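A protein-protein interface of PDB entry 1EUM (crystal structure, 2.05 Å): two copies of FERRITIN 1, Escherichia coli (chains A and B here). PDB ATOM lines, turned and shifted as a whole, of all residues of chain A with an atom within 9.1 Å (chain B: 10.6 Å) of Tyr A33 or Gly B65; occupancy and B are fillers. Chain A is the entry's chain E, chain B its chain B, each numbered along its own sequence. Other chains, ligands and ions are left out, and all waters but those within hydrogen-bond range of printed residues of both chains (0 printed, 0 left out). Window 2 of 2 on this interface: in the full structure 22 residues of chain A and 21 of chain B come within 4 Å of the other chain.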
ATOM      1  N   GLN A  26     -18.958  -3.877   9.650  1.00  0.00           N
ATOM      2  CA  GLN A  26     -19.153  -3.675   8.218  1.00  0.00           C
ATOM      3  C   GLN A  26     -19.075  -4.993   7.429  1.00  0.00           C
ATOM      4  O   GLN A  26     -19.791  -5.174   6.462  1.00  0.00           O
ATOM      5  CB  GLN A  26     -18.144  -2.663   7.676  1.00  0.00           C
ATOM      6  CG  GLN A  26     -18.348  -2.316   6.195  1.00  0.00           C
ATOM      7  CD  GLN A  26     -19.650  -1.583   5.943  1.00  0.00           C
ATOM      8  OE1 GLN A  26     -20.579  -2.133   5.356  1.00  0.00           O
ATOM      9  NE2 GLN A  26     -19.733  -0.343   6.411  1.00  0.00           N
ATOM     10  N   MET A  27     -18.200  -5.907   7.855  1.00  0.00           N
ATOM     11  CA  MET A  27     -18.063  -7.220   7.193  1.00  0.00           C
ATOM     12  C   MET A  27     -19.316  -8.069   7.437  1.00  0.00           C
ATOM     13  O   MET A  27     -19.713  -8.858   6.587  1.00  0.00           O
ATOM     14  CB  MET A  27     -16.839  -7.969   7.719  1.00  0.00           C
ATOM     15  CG  MET A  27     -15.536  -7.595   7.066  1.00  0.00           C
ATOM     16  SD  MET A  27     -14.174  -8.212   8.054  1.00  0.00           S
ATOM     17  CE  MET A  27     -12.791  -7.961   6.913  1.00  0.00           C
ATOM     18  N   SER A  28     -19.924  -7.905   8.614  1.00  0.00           N
ATOM     19  CA  SER A  28     -21.137  -8.629   8.941  1.00  0.00           C
ATOM     20  C   SER A  28     -22.226  -8.186   7.977  1.00  0.00           C
ATOM     21  O   SER A  28     -23.059  -8.982   7.558  1.00  0.00           O
ATOM     22  CB  SER A  28     -21.581  -8.347  10.389  1.00  0.00           C
ATOM     23  OG  SER A  28     -22.188  -7.080  10.495  1.00  0.00           O
ATOM     24  N   ALA A  29     -22.213  -6.907   7.625  1.00  0.00           N
ATOM     25  CA  ALA A  29     -23.185  -6.375   6.680  1.00  0.00           C
ATOM     26  C   ALA A  29     -23.032  -7.064   5.310  1.00  0.00           C
ATOM     27  O   ALA A  29     -24.018  -7.459   4.694  1.00  0.00           O
ATOM     28  CB  ALA A  29     -23.033  -4.860   6.553  1.00  0.00           C
ATOM     29  N   TRP A  30     -21.791  -7.235   4.859  1.00  0.00           N
ATOM     30  CA  TRP A  30     -21.527  -7.898   3.588  1.00  0.00           C
ATOM     31  C   TRP A  30     -22.109  -9.302   3.610  1.00  0.00           C
ATOM     32  O   TRP A  30     -22.791  -9.719   2.676  1.00  0.00           O
ATOM     33  CB  TRP A  30     -20.023  -7.970   3.333  1.00  0.00           C
ATOM     34  CG  TRP A  30     -19.676  -8.479   1.957  1.00  0.00           C
ATOM     35  CD1 TRP A  30     -19.448  -7.732   0.841  1.00  0.00           C
ATOM     36  CD2 TRP A  30     -19.526  -9.848   1.560  1.00  0.00           C
ATOM     37  NE1 TRP A  30     -19.149  -8.550  -0.225  1.00  0.00           N
ATOM     38  CE2 TRP A  30     -19.205  -9.853   0.187  1.00  0.00           C
ATOM     39  CE3 TRP A  30     -19.632 -11.067   2.234  1.00  0.00           C
ATOM     40  CZ2 TRP A  30     -18.979 -11.026  -0.520  1.00  0.00           C
ATOM     41  CZ3 TRP A  30     -19.418 -12.235   1.526  1.00  0.00           C
ATOM     42  CH2 TRP A  30     -19.099 -12.207   0.162  1.00  0.00           C
ATOM     43  N   CYS A  31     -21.854 -10.012   4.702  1.00  0.00           N
ATOM     44  CA  CYS A  31     -22.333 -11.372   4.867  1.00  0.00           C
ATOM     45  C   CYS A  31     -23.843 -11.484   4.752  1.00  0.00           C
ATOM     46  O   CYS A  31     -24.354 -12.297   3.992  1.00  0.00           O
ATOM     47  CB  CYS A  31     -21.848 -11.941   6.192  1.00  0.00           C
ATOM     48  SG  CYS A  31     -20.043 -12.217   6.220  1.00  0.00           S
ATOM     49  N   SER A  32     -24.553 -10.663   5.513  1.00  0.00           N
ATOM     50  CA  SER A  32     -26.013 -10.650   5.471  1.00  0.00           C
ATOM     51  C   SER A  32     -26.507 -10.342   4.052  1.00  0.00           C
ATOM     52  O   SER A  32     -27.373 -11.025   3.532  1.00  0.00           O
ATOM     53  CB  SER A  32     -26.562  -9.597   6.437  1.00  0.00           C
ATOM     54  OG  SER A  32     -26.465 -10.030   7.774  1.00  0.00           O
ATOM     55  N   TYR A  33     -25.945  -9.301   3.446  1.00  0.00           N
ATOM     56  CA  TYR A  33     -26.322  -8.905   2.099  1.00  0.00           C
ATOM     57  C   TYR A  33     -26.100 -10.040   1.120  1.00  0.00           C
ATOM     58  O   TYR A  33     -26.758 -10.099   0.088  1.00  0.00           O
ATOM     59  CB  TYR A  33     -25.533  -7.659   1.652  1.00  0.00           C
ATOM     60  CG  TYR A  33     -25.993  -7.072   0.329  1.00  0.00           C
ATOM     61  CD1 TYR A  33     -27.238  -6.464   0.216  1.00  0.00           C
ATOM     62  CD2 TYR A  33     -25.176  -7.105  -0.791  1.00  0.00           C
ATOM     63  CE1 TYR A  33     -27.658  -5.909  -0.976  1.00  0.00           C
ATOM     64  CE2 TYR A  33     -25.594  -6.568  -1.998  1.00  0.00           C
ATOM     65  CZ  TYR A  33     -26.836  -5.965  -2.082  1.00  0.00           C
ATOM     66  OH  TYR A  33     -27.248  -5.409  -3.268  1.00  0.00           O
ATOM     67  N   HIS A  34     -25.167 -10.937   1.446  1.00  0.00           N
ATOM     68  CA  HIS A  34     -24.853 -12.061   0.573  1.00  0.00           C
ATOM     69  C   HIS A  34     -25.413 -13.394   1.059  1.00  0.00           C
ATOM     70  O   HIS A  34     -25.018 -14.458   0.588  1.00  0.00           O
ATOM     71  CB  HIS A  34     -23.349 -12.135   0.255  1.00  0.00           C
ATOM     72  CG  HIS A  34     -22.849 -10.970  -0.548  1.00  0.00           C
ATOM     73  ND1 HIS A  34     -22.678 -11.023  -1.914  1.00  0.00           N
ATOM     74  CD2 HIS A  34     -22.499  -9.712  -0.175  1.00  0.00           C
ATOM     75  CE1 HIS A  34     -22.233  -9.853  -2.348  1.00  0.00           C
ATOM     76  NE2 HIS A  34     -22.120  -9.039  -1.313  1.00  0.00           N
ATOM     77  N   THR A  35     -26.374 -13.313   1.974  1.00  0.00           N
ATOM     78  CA  THR A  35     -27.092 -14.486   2.461  1.00  0.00           C
ATOM     79  C   THR A  35     -26.395 -15.364   3.467  1.00  0.00           C
ATOM     80  O   THR A  35     -26.859 -16.481   3.736  1.00  0.00           O
ATOM     81  CB  THR A  35     -27.620 -15.366   1.298  1.00  0.00           C
ATOM     82  OG1 THR A  35     -26.558 -16.187   0.792  1.00  0.00           O
ATOM     83  CG2 THR A  35     -28.151 -14.493   0.168  1.00  0.00           C
ATOM     84  N   PHE A  36     -25.302 -14.876   4.045  1.00  0.00           N
ATOM     85  CA  PHE A  36     -24.562 -15.652   5.042  1.00  0.00           C
ATOM     86  C   PHE A  36     -24.866 -15.132   6.436  1.00  0.00           C
ATOM     87  O   PHE A  36     -24.028 -14.503   7.079  1.00  0.00           O
ATOM     88  CB  PHE A  36     -23.065 -15.593   4.762  1.00  0.00           C
ATOM     89  CG  PHE A  36     -22.685 -16.138   3.420  1.00  0.00           C
ATOM     90  CD1 PHE A  36     -22.126 -15.317   2.455  1.00  0.00           C
ATOM     91  CD2 PHE A  36     -22.895 -17.474   3.120  1.00  0.00           C
ATOM     92  CE1 PHE A  36     -21.769 -15.821   1.224  1.00  0.00           C
ATOM     93  CE2 PHE A  36     -22.540 -17.986   1.886  1.00  0.00           C
ATOM     94  CZ  PHE A  36     -21.980 -17.159   0.938  1.00  0.00           C
ATOM     95  N   GLU A  37     -26.086 -15.385   6.884  1.00  0.00           N
ATOM     96  CA  GLU A  37     -26.564 -14.919   8.182  1.00  0.00           C
ATOM     97  C   GLU A  37     -25.775 -15.457   9.372  1.00  0.00           C
ATOM     98  O   GLU A  37     -25.656 -14.782  10.407  1.00  0.00           O
ATOM     99  CB  GLU A  37     -28.055 -15.232   8.342  1.00  0.00           C
ATOM    100  CG  GLU A  37     -28.932 -14.617   7.260  1.00  0.00           C
ATOM    101  CD  GLU A  37     -28.684 -13.122   7.086  1.00  0.00           C
ATOM    102  OE1 GLU A  37     -28.586 -12.661   5.918  1.00  0.00           O
ATOM    103  OE2 GLU A  37     -28.598 -12.409   8.118  1.00  0.00           O
ATOM    104  N   ALA A  40     -22.526 -13.626   9.420  1.00  0.00           N
ATOM    105  CA  ALA A  40     -22.890 -12.275   9.838  1.00  0.00           C
ATOM    106  C   ALA A  40     -23.044 -12.172  11.349  1.00  0.00           C
ATOM    107  O   ALA A  40     -22.549 -11.233  11.976  1.00  0.00           O
ATOM    108  CB  ALA A  40     -24.169 -11.827   9.142  1.00  0.00           C
ATOM    109  N   PHE A  77     -15.587   0.404   4.768  1.00  0.00           N
ATOM    110  CA  PHE A  77     -16.293  -0.119   3.626  1.00  0.00           C
ATOM    111  C   PHE A  77     -15.353  -0.704   2.584  1.00  0.00           C
ATOM    112  O   PHE A  77     -14.336  -0.100   2.248  1.00  0.00           O
ATOM    113  CB  PHE A  77     -17.180   0.939   2.991  1.00  0.00           C
ATOM    114  CG  PHE A  77     -18.019   0.411   1.869  1.00  0.00           C
ATOM    115  CD1 PHE A  77     -19.145  -0.347   2.135  1.00  0.00           C
ATOM    116  CD2 PHE A  77     -17.632   0.589   0.548  1.00  0.00           C
ATOM    117  CE1 PHE A  77     -19.900  -0.867   1.109  1.00  0.00           C
ATOM    118  CE2 PHE A  77     -18.385   0.070  -0.483  1.00  0.00           C
ATOM    119  CZ  PHE A  77     -19.526  -0.654  -0.209  1.00  0.00           C
ATOM    120  N   ALA A  78     -15.714  -1.878   2.069  1.00  0.00           N
ATOM    121  CA  ALA A  78     -14.917  -2.562   1.052  1.00  0.00           C
ATOM    122  C   ALA A  78     -15.768  -3.610   0.368  1.00  0.00           C
ATOM    123  O   ALA A  78     -16.881  -3.896   0.801  1.00  0.00           O
ATOM    124  CB  ALA A  78     -13.685  -3.219   1.687  1.00  0.00           C
ATOM    125  N   GLU A  79     -15.243  -4.175  -0.705  1.00  0.00           N
ATOM    126  CA  GLU A  79     -15.942  -5.215  -1.434  1.00  0.00           C
ATOM    127  C   GLU A  79     -15.149  -6.503  -1.342  1.00  0.00           C
ATOM    128  O   GLU A  79     -13.912  -6.489  -1.308  1.00  0.00           O
ATOM    129  CB  GLU A  79     -16.119  -4.823  -2.901  1.00  0.00           C
ATOM    130  CG  GLU A  79     -17.201  -5.616  -3.611  1.00  0.00           C
ATOM    131  CD  GLU A  79     -18.329  -6.020  -2.675  1.00  0.00           C
ATOM    132  OE1 GLU A  79     -18.891  -7.117  -2.860  1.00  0.00           O
ATOM    133  OE2 GLU A  79     -18.646  -5.238  -1.748  1.00  0.00           O
ATOM    134  N   TYR A  80     -15.857  -7.618  -1.302  1.00  0.00           N
ATOM    135  CA  TYR A  80     -15.210  -8.905  -1.208  1.00  0.00           C
ATOM    136  C   TYR A  80     -15.744  -9.801  -2.300  1.00  0.00           C
ATOM    137  O   TYR A  80     -16.918  -9.723  -2.655  1.00  0.00           O
ATOM    138  CB  TYR A  80     -15.471  -9.508   0.166  1.00  0.00           C
ATOM    139  CG  TYR A  80     -15.016  -8.605   1.277  1.00  0.00           C
ATOM    140  CD1 TYR A  80     -15.931  -7.893   2.039  1.00  0.00           C
ATOM    141  CD2 TYR A  80     -13.657  -8.405   1.518  1.00  0.00           C
ATOM    142  CE1 TYR A  80     -15.511  -7.030   3.051  1.00  0.00           C
ATOM    143  CE2 TYR A  80     -13.222  -7.547   2.525  1.00  0.00           C
ATOM    144  CZ  TYR A  80     -14.156  -6.860   3.285  1.00  0.00           C
ATOM    145  OH  TYR A  80     -13.730  -6.015   4.287  1.00  0.00           O
ATOM    146  N   LEU B   2     -37.652  -0.488  -0.020  1.00  0.00           N
ATOM    147  CA  LEU B   2     -37.324   0.872   0.385  1.00  0.00           C
ATOM    148  C   LEU B   2     -36.865   1.698  -0.798  1.00  0.00           C
ATOM    149  O   LEU B   2     -36.135   1.211  -1.663  1.00  0.00           O
ATOM    150  CB  LEU B   2     -36.213   0.861   1.439  1.00  0.00           C
ATOM    151  CG  LEU B   2     -36.570   0.342   2.830  1.00  0.00           C
ATOM    152  CD1 LEU B   2     -35.388   0.518   3.768  1.00  0.00           C
ATOM    153  CD2 LEU B   2     -37.782   1.050   3.369  1.00  0.00           C
ATOM    154  N   LYS B   3     -37.272   2.959  -0.822  1.00  0.00           N
ATOM    155  CA  LYS B   3     -36.838   3.876  -1.867  1.00  0.00           C
ATOM    156  C   LYS B   3     -35.398   4.298  -1.569  1.00  0.00           C
ATOM    157  O   LYS B   3     -34.992   4.348  -0.414  1.00  0.00           O
ATOM    158  CB  LYS B   3     -37.732   5.115  -1.880  1.00  0.00           C
ATOM    159  CG  LYS B   3     -39.111   4.875  -2.466  1.00  0.00           C
ATOM    160  CD  LYS B   3     -39.980   6.102  -2.327  1.00  0.00           C
ATOM    161  CE  LYS B   3     -40.391   6.649  -3.680  1.00  0.00           C
ATOM    162  NZ  LYS B   3     -39.987   8.073  -3.844  1.00  0.00           N
ATOM    163  N   ILE B   7     -33.374   4.722   2.063  1.00  0.00           N
ATOM    164  CA  ILE B   7     -32.206   3.925   2.406  1.00  0.00           C
ATOM    165  C   ILE B   7     -31.069   4.862   2.833  1.00  0.00           C
ATOM    166  O   ILE B   7     -30.405   4.642   3.848  1.00  0.00           O
ATOM    167  CB  ILE B   7     -31.748   3.072   1.213  1.00  0.00           C
ATOM    168  CG1 ILE B   7     -32.785   1.986   0.910  1.00  0.00           C
ATOM    169  CG2 ILE B   7     -30.362   2.446   1.485  1.00  0.00           C
ATOM    170  CD1 ILE B   7     -32.592   1.336  -0.460  1.00  0.00           C
ATOM    171  N   LEU B  10     -31.775   6.616   6.248  1.00  0.00           N
ATOM    172  CA  LEU B  10     -31.617   5.649   7.337  1.00  0.00           C
ATOM    173  C   LEU B  10     -30.133   5.397   7.560  1.00  0.00           C
ATOM    174  O   LEU B  10     -29.662   5.364   8.688  1.00  0.00           O
ATOM    175  CB  LEU B  10     -32.331   4.332   7.004  1.00  0.00           C
ATOM    176  CG  LEU B  10     -33.867   4.401   7.049  1.00  0.00           C
ATOM    177  CD1 LEU B  10     -34.507   3.212   6.371  1.00  0.00           C
ATOM    178  CD2 LEU B  10     -34.370   4.530   8.465  1.00  0.00           C
ATOM    179  N   LEU B  57     -30.837   0.409  13.678  1.00  0.00           N
ATOM    180  CA  LEU B  57     -30.946   0.967  12.328  1.00  0.00           C
ATOM    181  C   LEU B  57     -30.185   0.065  11.363  1.00  0.00           C
ATOM    182  O   LEU B  57     -30.638  -0.223  10.265  1.00  0.00           O
ATOM    183  CB  LEU B  57     -30.349   2.359  12.290  1.00  0.00           C
ATOM    184  CG  LEU B  57     -31.306   3.440  12.753  1.00  0.00           C
ATOM    185  CD1 LEU B  57     -30.524   4.657  13.239  1.00  0.00           C
ATOM    186  CD2 LEU B  57     -32.207   3.798  11.589  1.00  0.00           C
ATOM    187  N   PHE B  58     -29.024  -0.388  11.806  1.00  0.00           N
ATOM    188  CA  PHE B  58     -28.203  -1.301  11.041  1.00  0.00           C
ATOM    189  C   PHE B  58     -29.043  -2.535  10.680  1.00  0.00           C
ATOM    190  O   PHE B  58     -29.101  -2.933   9.519  1.00  0.00           O
ATOM    191  CB  PHE B  58     -26.991  -1.711  11.901  1.00  0.00           C
ATOM    192  CG  PHE B  58     -25.946  -2.531  11.168  1.00  0.00           C
ATOM    193  CD1 PHE B  58     -26.034  -3.928  11.123  1.00  0.00           C
ATOM    194  CD2 PHE B  58     -24.820  -1.915  10.609  1.00  0.00           C
ATOM    195  CE1 PHE B  58     -25.050  -4.688  10.484  1.00  0.00           C
ATOM    196  CE2 PHE B  58     -23.827  -2.674   9.968  1.00  0.00           C
ATOM    197  CZ  PHE B  58     -23.948  -4.055   9.904  1.00  0.00           C
ATOM    198  N   ASP B  59     -29.699  -3.126  11.682  1.00  0.00           N
ATOM    199  CA  ASP B  59     -30.545  -4.320  11.475  1.00  0.00           C
ATOM    200  C   ASP B  59     -31.732  -4.061  10.560  1.00  0.00           C
ATOM    201  O   ASP B  59     -32.090  -4.902   9.742  1.00  0.00           O
ATOM    202  CB  ASP B  59     -31.053  -4.844  12.797  1.00  0.00           C
ATOM    203  CG  ASP B  59     -29.955  -5.408  13.656  1.00  0.00           C
ATOM    204  OD1 ASP B  59     -30.197  -5.589  14.866  1.00  0.00           O
ATOM    205  OD2 ASP B  59     -28.851  -5.666  13.126  1.00  0.00           O
ATOM    206  N   TYR B  60     -32.372  -2.913  10.713  1.00  0.00           N
ATOM    207  CA  TYR B  60     -33.502  -2.615   9.854  1.00  0.00           C
ATOM    208  C   TYR B  60     -33.027  -2.579   8.398  1.00  0.00           C
ATOM    209  O   TYR B  60     -33.718  -3.055   7.505  1.00  0.00           O
ATOM    210  CB  TYR B  60     -34.193  -1.304  10.260  1.00  0.00           C
ATOM    211  CG  TYR B  60     -35.401  -0.955   9.414  1.00  0.00           C
ATOM    212  CD1 TYR B  60     -36.617  -1.582   9.617  1.00  0.00           C
ATOM    213  CD2 TYR B  60     -35.326   0.002   8.421  1.00  0.00           C
ATOM    214  CE1 TYR B  60     -37.730  -1.268   8.844  1.00  0.00           C
ATOM    215  CE2 TYR B  60     -36.428   0.319   7.648  1.00  0.00           C
ATOM    216  CZ  TYR B  60     -37.630  -0.321   7.870  1.00  0.00           C
ATOM    217  OH  TYR B  60     -38.733  -0.014   7.104  1.00  0.00           O
ATOM    218  N   LEU B  61     -31.828  -2.044   8.166  1.00  0.00           N
ATOM    219  CA  LEU B  61     -31.289  -1.972   6.808  1.00  0.00           C
ATOM    220  C   LEU B  61     -30.981  -3.355   6.228  1.00  0.00           C
ATOM    221  O   LEU B  61     -31.279  -3.624   5.061  1.00  0.00           O
ATOM    222  CB  LEU B  61     -30.061  -1.060   6.738  1.00  0.00           C
ATOM    223  CG  LEU B  61     -30.400   0.437   6.694  1.00  0.00           C
ATOM    224  CD1 LEU B  61     -29.167   1.306   6.898  1.00  0.00           C
ATOM    225  CD2 LEU B  61     -31.094   0.788   5.399  1.00  0.00           C
ATOM    226  N   THR B  62     -30.423  -4.245   7.050  1.00  0.00           N
ATOM    227  CA  THR B  62     -30.119  -5.598   6.583  1.00  0.00           C
ATOM    228  C   THR B  62     -31.389  -6.437   6.398  1.00  0.00           C
ATOM    229  O   THR B  62     -31.480  -7.205   5.460  1.00  0.00           O
ATOM    230  CB  THR B  62     -29.118  -6.335   7.498  1.00  0.00           C
ATOM    231  OG1 THR B  62     -29.565  -6.275   8.845  1.00  0.00           O
ATOM    232  CG2 THR B  62     -27.746  -5.702   7.406  1.00  0.00           C
ATOM    233  N   ASP B  63     -32.379  -6.242   7.273  1.00  0.00           N
ATOM    234  CA  ASP B  63     -33.654  -6.975   7.191  1.00  0.00           C
ATOM    235  C   ASP B  63     -34.382  -6.699   5.896  1.00  0.00           C
ATOM    236  O   ASP B  63     -35.105  -7.548   5.389  1.00  0.00           O
ATOM    237  CB  ASP B  63     -34.596  -6.576   8.334  1.00  0.00           C
ATOM    238  CG  ASP B  63     -34.246  -7.246   9.634  1.00  0.00           C
ATOM    239  OD1 ASP B  63     -33.256  -8.005   9.669  1.00  0.00           O
ATOM    240  OD2 ASP B  63     -34.925  -6.939  10.645  1.00  0.00           O
ATOM    241  N   THR B  64     -34.233  -5.484   5.394  1.00  0.00           N
ATOM    242  CA  THR B  64     -34.905  -5.076   4.179  1.00  0.00           C
ATOM    243  C   THR B  64     -34.099  -5.351   2.918  1.00  0.00           C
ATOM    244  O   THR B  64     -34.467  -4.916   1.831  1.00  0.00           O
ATOM    245  CB  THR B  64     -35.342  -3.608   4.245  1.00  0.00           C
ATOM    246  OG1 THR B  64     -34.191  -2.763   4.362  1.00  0.00           O
ATOM    247  CG2 THR B  64     -36.225  -3.392   5.432  1.00  0.00           C
ATOM    248  N   GLY B  65     -33.008  -6.100   3.061  1.00  0.00           N
ATOM    249  CA  GLY B  65     -32.175  -6.470   1.914  1.00  0.00           C
ATOM    250  C   GLY B  65     -31.233  -5.366   1.428  1.00  0.00           C
ATOM    251  O   GLY B  65     -30.871  -5.313   0.251  1.00  0.00           O
ATOM    252  N   ASN B  66     -30.816  -4.498   2.328  1.00  0.00           N
ATOM    253  CA  ASN B  66     -29.917  -3.436   1.956  1.00  0.00           C
ATOM    254  C   ASN B  66     -28.584  -3.589   2.626  1.00  0.00           C
ATOM    255  O   ASN B  66     -28.412  -4.429   3.491  1.00  0.00           O
ATOM    256  CB  ASN B  66     -30.531  -2.087   2.258  1.00  0.00           C
ATOM    257  CG  ASN B  66     -31.789  -1.852   1.459  1.00  0.00           C
ATOM    258  OD1 ASN B  66     -31.741  -1.744   0.229  1.00  0.00           O
ATOM    259  ND2 ASN B  66     -32.935  -1.861   2.136  1.00  0.00           N
ATOM    260  N   LEU B  67     -27.620  -2.790   2.200  1.00  0.00           N
ATOM    261  CA  LEU B  67     -26.282  -2.882   2.741  1.00  0.00           C
ATOM    262  C   LEU B  67     -25.883  -1.620   3.475  1.00  0.00           C
ATOM    263  O   LEU B  67     -25.540  -0.617   2.859  1.00  0.00           O
ATOM    264  CB  LEU B  67     -25.293  -3.167   1.611  1.00  0.00           C
ATOM    265  CG  LEU B  67     -23.824  -3.353   1.954  1.00  0.00           C
ATOM    266  CD1 LEU B  67     -23.674  -4.424   3.016  1.00  0.00           C
ATOM    267  CD2 LEU B  67     -23.072  -3.726   0.700  1.00  0.00           C
ATOM    268  N   PRO B  68     -25.937  -1.665   4.795  1.00  0.00           N
ATOM    269  CA  PRO B  68     -25.531  -0.512   5.585  1.00  0.00           C
ATOM    270  C   PRO B  68     -24.064  -0.197   5.285  1.00  0.00           C
ATOM    271  O   PRO B  68     -23.258  -1.089   5.053  1.00  0.00           O
ATOM    272  CB  PRO B  68     -25.700  -0.978   7.045  1.00  0.00           C
ATOM    273  CG  PRO B  68     -26.097  -2.394   7.004  1.00  0.00           C
ATOM    274  CD  PRO B  68     -26.317  -2.833   5.607  1.00  0.00           C
ATOM    275  N   ARG B  69     -23.732   1.075   5.276  1.00  0.00           N
ATOM    276  CA  ARG B  69     -22.380   1.479   5.022  1.00  0.00           C
ATOM    277  C   ARG B  69     -21.908   2.461   6.089  1.00  0.00           C
ATOM    278  O   ARG B  69     -22.471   3.543   6.248  1.00  0.00           O
ATOM    279  CB  ARG B  69     -22.257   2.108   3.642  1.00  0.00           C
ATOM    280  CG  ARG B  69     -20.866   2.655   3.339  1.00  0.00           C
ATOM    281  CD  ARG B  69     -20.842   3.480   2.061  1.00  0.00           C
ATOM    282  NE  ARG B  69     -21.798   4.590   2.116  1.00  0.00           N
ATOM    283  CZ  ARG B  69     -22.952   4.595   1.462  1.00  0.00           C
ATOM    284  NH1 ARG B  69     -23.757   5.630   1.580  1.00  0.00           N
ATOM    285  NH2 ARG B  69     -23.293   3.569   0.689  1.00  0.00           N
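No position is printed for both chains.
Arg B69 touches Gln A26 (CA to NE2, 3.5 Å).
Phe B58 touches Ser A28.
Phe B58 touches Ala A29.
CD1 of Leu B67 touches O of Ala A29, 3.5 Å away.
Ala A29 touches Pro B68 (CB to CG, 3.96 Å).
Leu B67 touches Trp A30.
Gly B65 touches Tyr A33.
CD1 of Tyr A33 touches C of Asn B66, at 3.99 Å.
Leu B67 touches Tyr A33.
Phe A77 touches Arg B69 (CD1 to CG, 3.7 Å).
OG1 of Thr B62 sits at hydrogen-bond distance from O of Phe B58 (3.4 Å).
O of Leu B61 lies within hydrogen-bond range of N of Asn B66 (2.9 Å).
ND2 of Asn B66 is in hydrogen-bond range of OG1 of Thr B64, at 2.7 Å.
A ring nitrogen (NE2) of His A34 sits at hydrogen-bond distance from the indole nitrogen (NE1) of Trp A30 (3.2 Å).
The indole nitrogen (NE1) of Trp A30 is in hydrogen-bond range of the side-chain carboxylate (OE1) of Glu A79, at 3.0 Å.
Printed residues of chain B that touch a printed residue of chain A: Phe B58, Gly B65, Asn B66, Leu B67, Pro B68 and Arg B69.
Hydrophobic or aromatic side chains of chain A that line the printed part of chain B: Ala A29, Tyr A33 and Phe A77.
The backbone carbonyl oxygen of Pro B68 sits close to the side-chain amide oxygen of Gln A26, 2.9 Å away.
Of the printed residues of chain B, Tyr A33 touches Gly B65 (3.5 Å), Asn B66 (3.99 Å) and Leu B67 (3.97 Å).
Gly B65 touches one residue of chain A.
Ala A29 touches three residues of chain B.
Ser A32 touches none of the printed residues of chain B.
His A34 touches none of the printed residues of chain B.
No residue of chain A comes within 4 Å of Thr B64.
Of the printed residues of chain B, Ser A28 touches Phe B58 (3.5 Å).
Printed residues of chain A within 4 Å of Asn B66: Tyr A33.
Printed residues of chain A within 4 Å of Phe B58: Ser A28 and Ala A29.
Of the printed residues of chain A, Arg B69 touches Gln A26 (3.5 Å) and Phe A77 (3.7 Å).
Cys A31 touches none of the printed residues of chain B.
Ala A78 touches none of the printed residues of chain B.
The nearest printed residue of chain B that does not touch Tyr A33 is Thr B62 (5.6 Å).
The nearest printed residue of chain B that does not touch Gln A26 is Leu B67 (4.5 Å).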
